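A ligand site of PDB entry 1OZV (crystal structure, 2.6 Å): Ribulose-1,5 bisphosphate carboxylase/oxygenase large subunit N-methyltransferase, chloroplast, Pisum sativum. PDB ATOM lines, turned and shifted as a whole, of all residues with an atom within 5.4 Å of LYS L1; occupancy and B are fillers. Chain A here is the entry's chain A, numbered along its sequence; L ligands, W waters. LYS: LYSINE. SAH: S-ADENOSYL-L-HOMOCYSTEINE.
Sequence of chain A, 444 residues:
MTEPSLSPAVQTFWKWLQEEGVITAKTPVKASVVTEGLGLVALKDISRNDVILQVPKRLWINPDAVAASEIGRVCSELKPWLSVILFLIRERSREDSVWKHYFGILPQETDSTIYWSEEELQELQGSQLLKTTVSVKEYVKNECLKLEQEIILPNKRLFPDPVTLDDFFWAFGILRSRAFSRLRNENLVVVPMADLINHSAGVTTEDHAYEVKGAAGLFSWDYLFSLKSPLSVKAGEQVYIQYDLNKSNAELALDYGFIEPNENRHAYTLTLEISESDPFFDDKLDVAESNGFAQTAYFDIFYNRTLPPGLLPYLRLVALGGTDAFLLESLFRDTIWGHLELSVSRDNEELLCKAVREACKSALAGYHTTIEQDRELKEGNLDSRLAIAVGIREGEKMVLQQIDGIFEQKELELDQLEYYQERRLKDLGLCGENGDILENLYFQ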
ATOM      1  N   SER A 177      -4.806 -17.769 -31.909  1.00  0.00           N
ATOM      2  CA  SER A 177      -6.057 -18.017 -31.204  1.00  0.00           C
ATOM      3  C   SER A 177      -6.262 -19.480 -30.832  1.00  0.00           C
ATOM      4  O   SER A 177      -7.208 -19.828 -30.121  1.00  0.00           O
ATOM      5  CB  SER A 177      -7.251 -17.528 -32.047  1.00  0.00           C
ATOM      6  OG  SER A 177      -7.313 -18.179 -33.306  1.00  0.00           O
ATOM      7  N   ARG A 178      -5.362 -20.344 -31.296  1.00  0.00           N
ATOM      8  CA  ARG A 178      -5.493 -21.760 -31.012  1.00  0.00           C
ATOM      9  C   ARG A 178      -4.390 -22.439 -30.196  1.00  0.00           C
ATOM     10  O   ARG A 178      -4.672 -23.145 -29.230  1.00  0.00           O
ATOM     11  CB  ARG A 178      -5.676 -22.520 -32.323  1.00  0.00           C
ATOM     12  CG  ARG A 178      -6.976 -22.197 -33.005  1.00  0.00           C
ATOM     13  CD  ARG A 178      -7.218 -23.164 -34.143  1.00  0.00           C
ATOM     14  NE  ARG A 178      -8.605 -23.126 -34.590  1.00  0.00           N
ATOM     15  CZ  ARG A 178      -9.627 -23.595 -33.896  1.00  0.00           C
ATOM     16  NH1 ARG A 178      -9.453 -24.138 -32.706  1.00  0.00           N
ATOM     17  NH2 ARG A 178     -10.859 -23.521 -34.393  1.00  0.00           N
ATOM     18  N   ALA A 179      -3.134 -22.242 -30.594  1.00  0.00           N
ATOM     19  CA  ALA A 179      -1.996 -22.851 -29.920  1.00  0.00           C
ATOM     20  C   ALA A 179      -1.924 -22.621 -28.407  1.00  0.00           C
ATOM     21  O   ALA A 179      -2.446 -21.638 -27.887  1.00  0.00           O
ATOM     22  CB  ALA A 179      -0.711 -22.372 -30.558  1.00  0.00           C
ATOM     23  N   PHE A 180      -1.282 -23.547 -27.709  1.00  0.00           N
ATOM     24  CA  PHE A 180      -1.113 -23.441 -26.264  1.00  0.00           C
ATOM     25  C   PHE A 180       0.327 -23.079 -25.995  1.00  0.00           C
ATOM     26  O   PHE A 180       1.213 -23.929 -26.028  1.00  0.00           O
ATOM     27  CB  PHE A 180      -1.446 -24.759 -25.572  1.00  0.00           C
ATOM     28  CG  PHE A 180      -2.841 -25.256 -25.839  1.00  0.00           C
ATOM     29  CD1 PHE A 180      -3.158 -25.832 -27.068  1.00  0.00           C
ATOM     30  CD2 PHE A 180      -3.830 -25.144 -24.881  1.00  0.00           C
ATOM     31  CE1 PHE A 180      -4.449 -26.297 -27.322  1.00  0.00           C
ATOM     32  CE2 PHE A 180      -5.119 -25.601 -25.123  1.00  0.00           C
ATOM     33  CZ  PHE A 180      -5.428 -26.181 -26.341  1.00  0.00           C
ATOM     34  N   SER A 181       0.568 -21.807 -25.739  1.00  0.00           N
ATOM     35  CA  SER A 181       1.925 -21.319 -25.485  1.00  0.00           C
ATOM     36  C   SER A 181       2.383 -21.561 -24.056  1.00  0.00           C
ATOM     37  O   SER A 181       3.571 -21.767 -23.816  1.00  0.00           O
ATOM     38  CB  SER A 181       2.003 -19.824 -25.798  1.00  0.00           C
ATOM     39  OG  SER A 181       1.024 -19.087 -25.066  1.00  0.00           O
ATOM     40  N   ARG A 182       1.448 -21.539 -23.120  1.00  0.00           N
ATOM     41  CA  ARG A 182       1.784 -21.750 -21.719  1.00  0.00           C
ATOM     42  C   ARG A 182       2.094 -23.226 -21.472  1.00  0.00           C
ATOM     43  O   ARG A 182       1.235 -24.010 -21.095  1.00  0.00           O
ATOM     44  CB  ARG A 182       0.627 -21.292 -20.814  1.00  0.00           C
ATOM     45  CG  ARG A 182       1.055 -20.970 -19.387  1.00  0.00           C
ATOM     46  CD  ARG A 182      -0.077 -20.387 -18.548  1.00  0.00           C
ATOM     47  NE  ARG A 182      -0.506 -19.067 -19.016  1.00  0.00           N
ATOM     48  CZ  ARG A 182      -1.347 -18.859 -20.020  1.00  0.00           C
ATOM     49  NH1 ARG A 182      -1.883 -19.883 -20.678  1.00  0.00           N
ATOM     50  NH2 ARG A 182      -1.659 -17.622 -20.378  1.00  0.00           N
ATOM     51  N   ALA A 194      -8.066 -30.964 -28.205  1.00  0.00           N
ATOM     52  CA  ALA A 194      -8.257 -29.944 -27.176  1.00  0.00           C
ATOM     53  C   ALA A 194      -8.172 -28.534 -27.781  1.00  0.00           C
ATOM     54  O   ALA A 194      -7.969 -27.551 -27.068  1.00  0.00           O
ATOM     55  CB  ALA A 194      -7.192 -30.114 -26.095  1.00  0.00           C
ATOM     56  N   ASP A 195      -8.339 -28.443 -29.087  1.00  0.00           N
ATOM     57  CA  ASP A 195      -8.290 -27.178 -29.792  1.00  0.00           C
ATOM     58  C   ASP A 195      -9.629 -26.468 -29.606  1.00  0.00           C
ATOM     59  O   ASP A 195      -9.693 -25.265 -29.419  1.00  0.00           O
ATOM     60  CB  ASP A 195      -8.028 -27.458 -31.279  1.00  0.00           C
ATOM     61  CG  ASP A 195      -7.475 -26.261 -32.015  1.00  0.00           C
ATOM     62  OD1 ASP A 195      -6.437 -25.711 -31.580  1.00  0.00           O
ATOM     63  OD2 ASP A 195      -8.068 -25.881 -33.049  1.00  0.00           O
ATOM     64  N   LEU A 196     -10.694 -27.275 -29.644  1.00  0.00           N
ATOM     65  CA  LEU A 196     -12.073 -26.807 -29.506  1.00  0.00           C
ATOM     66  C   LEU A 196     -12.482 -26.303 -28.121  1.00  0.00           C
ATOM     67  O   LEU A 196     -13.590 -25.781 -27.951  1.00  0.00           O
ATOM     68  CB  LEU A 196     -13.023 -27.925 -29.927  1.00  0.00           C
ATOM     69  CG  LEU A 196     -12.798 -28.475 -31.329  1.00  0.00           C
ATOM     70  CD1 LEU A 196     -13.629 -29.721 -31.512  1.00  0.00           C
ATOM     71  CD2 LEU A 196     -13.177 -27.426 -32.365  1.00  0.00           C
ATOM     72  N   ILE A 197     -11.609 -26.456 -27.126  1.00  0.00           N
ATOM     73  CA  ILE A 197     -11.903 -26.007 -25.764  1.00  0.00           C
ATOM     74  C   ILE A 197     -12.049 -24.475 -25.772  1.00  0.00           C
ATOM     75  O   ILE A 197     -11.180 -23.758 -26.277  1.00  0.00           O
ATOM     76  CB  ILE A 197     -10.764 -26.426 -24.806  1.00  0.00           C
ATOM     77  CG1 ILE A 197     -11.169 -26.204 -23.352  1.00  0.00           C
ATOM     78  CG2 ILE A 197      -9.506 -25.630 -25.122  1.00  0.00           C
ATOM     79  CD1 ILE A 197     -12.156 -27.210 -22.841  1.00  0.00           C
ATOM     80  N   TYR A 210      -3.727 -28.031 -19.024  1.00  0.00           N
ATOM     81  CA  TYR A 210      -3.071 -29.064 -19.800  1.00  0.00           C
ATOM     82  C   TYR A 210      -1.660 -29.374 -19.303  1.00  0.00           C
ATOM     83  O   TYR A 210      -0.934 -28.495 -18.844  1.00  0.00           O
ATOM     84  CB  TYR A 210      -3.043 -28.672 -21.282  1.00  0.00           C
ATOM     85  CG  TYR A 210      -2.480 -27.288 -21.566  1.00  0.00           C
ATOM     86  CD1 TYR A 210      -1.147 -27.127 -21.943  1.00  0.00           C
ATOM     87  CD2 TYR A 210      -3.270 -26.154 -21.461  1.00  0.00           C
ATOM     88  CE1 TYR A 210      -0.623 -25.862 -22.224  1.00  0.00           C
ATOM     89  CE2 TYR A 210      -2.766 -24.884 -21.734  1.00  0.00           C
ATOM     90  CZ  TYR A 210      -1.443 -24.750 -22.116  1.00  0.00           C
ATOM     91  OH  TYR A 210      -0.941 -23.497 -22.394  1.00  0.00           O
ATOM     92  N   ILE A 241     -12.075 -23.263 -20.044  1.00  0.00           N
ATOM     93  CA  ILE A 241     -10.760 -23.060 -19.450  1.00  0.00           C
ATOM     94  C   ILE A 241     -10.460 -21.561 -19.460  1.00  0.00           C
ATOM     95  O   ILE A 241     -11.154 -20.785 -20.112  1.00  0.00           O
ATOM     96  CB  ILE A 241      -9.642 -23.751 -20.253  1.00  0.00           C
ATOM     97  CG1 ILE A 241      -9.674 -23.263 -21.706  1.00  0.00           C
ATOM     98  CG2 ILE A 241      -9.785 -25.259 -20.165  1.00  0.00           C
ATOM     99  CD1 ILE A 241      -8.495 -23.723 -22.526  1.00  0.00           C
ATOM    100  N   TYR A 243      -8.141 -18.860 -20.764  1.00  0.00           N
ATOM    101  CA  TYR A 243      -7.061 -18.603 -21.702  1.00  0.00           C
ATOM    102  C   TYR A 243      -5.894 -17.805 -21.105  1.00  0.00           C
ATOM    103  O   TYR A 243      -4.741 -18.107 -21.378  1.00  0.00           O
ATOM    104  CB  TYR A 243      -7.583 -17.883 -22.962  1.00  0.00           C
ATOM    105  CG  TYR A 243      -8.382 -18.752 -23.907  1.00  0.00           C
ATOM    106  CD1 TYR A 243      -8.866 -18.236 -25.108  1.00  0.00           C
ATOM    107  CD2 TYR A 243      -8.674 -20.081 -23.590  1.00  0.00           C
ATOM    108  CE1 TYR A 243      -9.623 -19.025 -25.975  1.00  0.00           C
ATOM    109  CE2 TYR A 243      -9.439 -20.882 -24.458  1.00  0.00           C
ATOM    110  CZ  TYR A 243      -9.913 -20.346 -25.647  1.00  0.00           C
ATOM    111  OH  TYR A 243     -10.634 -21.135 -26.513  1.00  0.00           O
ATOM    112  N   LYS A 247      -4.027 -11.065 -19.375  1.00  0.00           N
ATOM    113  CA  LYS A 247      -4.237 -10.273 -20.578  1.00  0.00           C
ATOM    114  C   LYS A 247      -5.302  -9.201 -20.377  1.00  0.00           C
ATOM    115  O   LYS A 247      -6.188  -9.332 -19.533  1.00  0.00           O
ATOM    116  CB  LYS A 247      -4.626 -11.150 -21.766  1.00  0.00           C
ATOM    117  CG  LYS A 247      -3.422 -11.766 -22.478  1.00  0.00           C
ATOM    118  CD  LYS A 247      -3.859 -12.733 -23.568  1.00  0.00           C
ATOM    119  CE  LYS A 247      -2.654 -13.439 -24.200  1.00  0.00           C
ATOM    120  NZ  LYS A 247      -3.071 -14.610 -25.043  1.00  0.00           N
ATOM    121  N   TYR A 256      -7.820 -13.328 -29.791  1.00  0.00           N
ATOM    122  CA  TYR A 256      -8.998 -14.127 -30.131  1.00  0.00           C
ATOM    123  C   TYR A 256     -10.004 -13.056 -30.516  1.00  0.00           C
ATOM    124  O   TYR A 256      -9.689 -11.866 -30.458  1.00  0.00           O
ATOM    125  CB  TYR A 256      -9.514 -14.914 -28.923  1.00  0.00           C
ATOM    126  CG  TYR A 256      -8.414 -15.349 -27.990  1.00  0.00           C
ATOM    127  CD1 TYR A 256      -8.050 -14.574 -26.893  1.00  0.00           C
ATOM    128  CD2 TYR A 256      -7.675 -16.517 -28.230  1.00  0.00           C
ATOM    129  CE1 TYR A 256      -6.990 -14.921 -26.078  1.00  0.00           C
ATOM    130  CE2 TYR A 256      -6.595 -16.878 -27.417  1.00  0.00           C
ATOM    131  CZ  TYR A 256      -6.266 -16.079 -26.340  1.00  0.00           C
ATOM    132  OH  TYR A 256      -5.191 -16.395 -25.550  1.00  0.00           O
HETATM  133  N   LYS L   1      -3.921 -18.992 -25.128  1.00  0.00           N
HETATM  134  CA  LYS L   1      -4.141 -20.187 -24.261  1.00  0.00           C
HETATM  135  C   LYS L   1      -2.832 -20.598 -23.615  1.00  0.00           C
HETATM  136  O   LYS L   1      -1.888 -19.774 -23.658  1.00  0.00           O
HETATM  137  CB  LYS L   1      -4.685 -21.356 -25.086  1.00  0.00           C
HETATM  138  CG  LYS L   1      -5.892 -21.029 -25.933  1.00  0.00           C
HETATM  139  CD  LYS L   1      -6.410 -22.268 -26.650  1.00  0.00           C
HETATM  140  CE  LYS L   1      -7.509 -21.923 -27.641  1.00  0.00           C
HETATM  141  NZ  LYS L   1      -8.166 -23.149 -28.189  1.00  0.00           N
HETATM  142  OXT LYS L   1      -2.763 -21.723 -23.072  1.00  0.00           O
HETATM  143  N   SAH L   2     -14.861 -22.426 -30.634  1.00  0.00           N
HETATM  144  CA  SAH L   2     -13.726 -22.542 -31.560  1.00  0.00           C
HETATM  145  CB  SAH L   2     -12.584 -23.360 -30.887  1.00  0.00           C
HETATM  146  CG  SAH L   2     -11.834 -22.646 -29.798  1.00  0.00           C
HETATM  147  SD  SAH L   2     -10.273 -21.788 -30.277  1.00  0.00           S
HETATM  148  C   SAH L   2     -14.174 -23.173 -32.922  1.00  0.00           C
HETATM  149  O   SAH L   2     -13.308 -23.536 -33.753  1.00  0.00           O
HETATM  150  OXT SAH L   2     -15.382 -23.317 -33.189  1.00  0.00           O
HETATM  151  C5' SAH L   2     -10.639 -20.170 -29.603  1.00  0.00           C
HETATM  152  C4' SAH L   2     -11.534 -19.321 -30.485  1.00  0.00           C
HETATM  153  O4' SAH L   2     -12.933 -19.633 -30.219  1.00  0.00           O
HETATM  154  C3' SAH L   2     -11.416 -17.825 -30.229  1.00  0.00           C
HETATM  155  O3' SAH L   2     -10.432 -17.227 -31.070  1.00  0.00           O
HETATM  156  C2' SAH L   2     -12.811 -17.285 -30.472  1.00  0.00           C
HETATM  157  O2' SAH L   2     -13.137 -16.878 -31.786  1.00  0.00           O
HETATM  158  C1' SAH L   2     -13.649 -18.443 -29.911  1.00  0.00           C
HETATM  159  N9  SAH L   2     -13.893 -18.333 -28.456  1.00  0.00           N
HETATM  160  C8  SAH L   2     -13.293 -19.008 -27.388  1.00  0.00           C
HETATM  161  N7  SAH L   2     -13.736 -18.675 -26.209  1.00  0.00           N
HETATM  162  C5  SAH L   2     -14.691 -17.710 -26.482  1.00  0.00           C
HETATM  163  C6  SAH L   2     -15.560 -16.965 -25.651  1.00  0.00           C
HETATM  164  N6  SAH L   2     -15.555 -17.062 -24.323  1.00  0.00           N
HETATM  165  N1  SAH L   2     -16.423 -16.068 -26.240  1.00  0.00           N
HETATM  166  C2  SAH L   2     -16.442 -15.953 -27.595  1.00  0.00           C
HETATM  167  N3  SAH L   2     -15.666 -16.621 -28.494  1.00  0.00           N
HETATM  168  C4  SAH L   2     -14.820 -17.504 -27.868  1.00  0.00           C
HETATM  169  O   HOH W   1      -1.390 -19.435 -26.889  1.00  0.00           O
HETATM  170  O   HOH W   2      -2.757 -17.375 -27.981  1.00  0.00           O
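OH of Tyr 210 lies within hydrogen-bond range of OXT of LYS L1, at 2.6 Å.
O of Asp 195 is in hydrogen-bond range of NZ of LYS L1.
OH of Tyr 256 lies within hydrogen-bond range of N of LYS L1 (2.9 Å).
The guanidinium group (NH1) of Arg 182 is in salt-bridge range of an oxygen (O) of LYS L1, 3.0 Å away.
O of LYS L1 lies within hydrogen-bond range of OG of Ser 181, 3.3 Å away.
An oxygen (O) of SAH L2 is in salt-bridge range of the guanidinium group of Arg 178, at 2.5 Å.
A nitrogen (NZ) of LYS L1 sits close to a sulfur (SD) of SAH L2 (3.3 Å).
The backbone carbonyl oxygen (O) of Arg 182 sits at hydrogen-bond distance from the side-chain hydroxyl (OH) of Tyr 210 (2.6 Å).
The side-chain carboxylate of Asp 195 is in salt-bridge range of the guanidinium group of Arg 178 (3.2 Å).
The side-chain amino group (NZ) of Lys 247 lies within hydrogen-bond range of the side-chain hydroxyl (OH) of Tyr 256 (2.8 Å).
The guanidinium group (NH2) of Arg 182 lies within hydrogen-bond range of the backbone carbonyl oxygen (O) of Tyr 243 (3.3 Å).
The side-chain hydroxyl (OH) of Tyr 243 is in hydrogen-bond range of the backbone carbonyl oxygen (O) of Ile 197.
Merely in contact with LYS L1: Arg 178 (3.2 Å), Ser 177 (3.3 Å), Tyr 243 (3.4 Å), Ala 179 (3.6 Å), Ile 197 (3.6 Å) and Phe 180 (3.9 Å).
Hydrophobic or aromatic side chains within 4 Å of LYS L1: Phe 180, Tyr 210, Tyr 243 and Tyr 256.
Water W1 lies within hydrogen-bond range of O of Ala 179 (2.6 Å), OG of Ser 181 (3.0 Å) and N of LYS L1 (3.1 Å).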
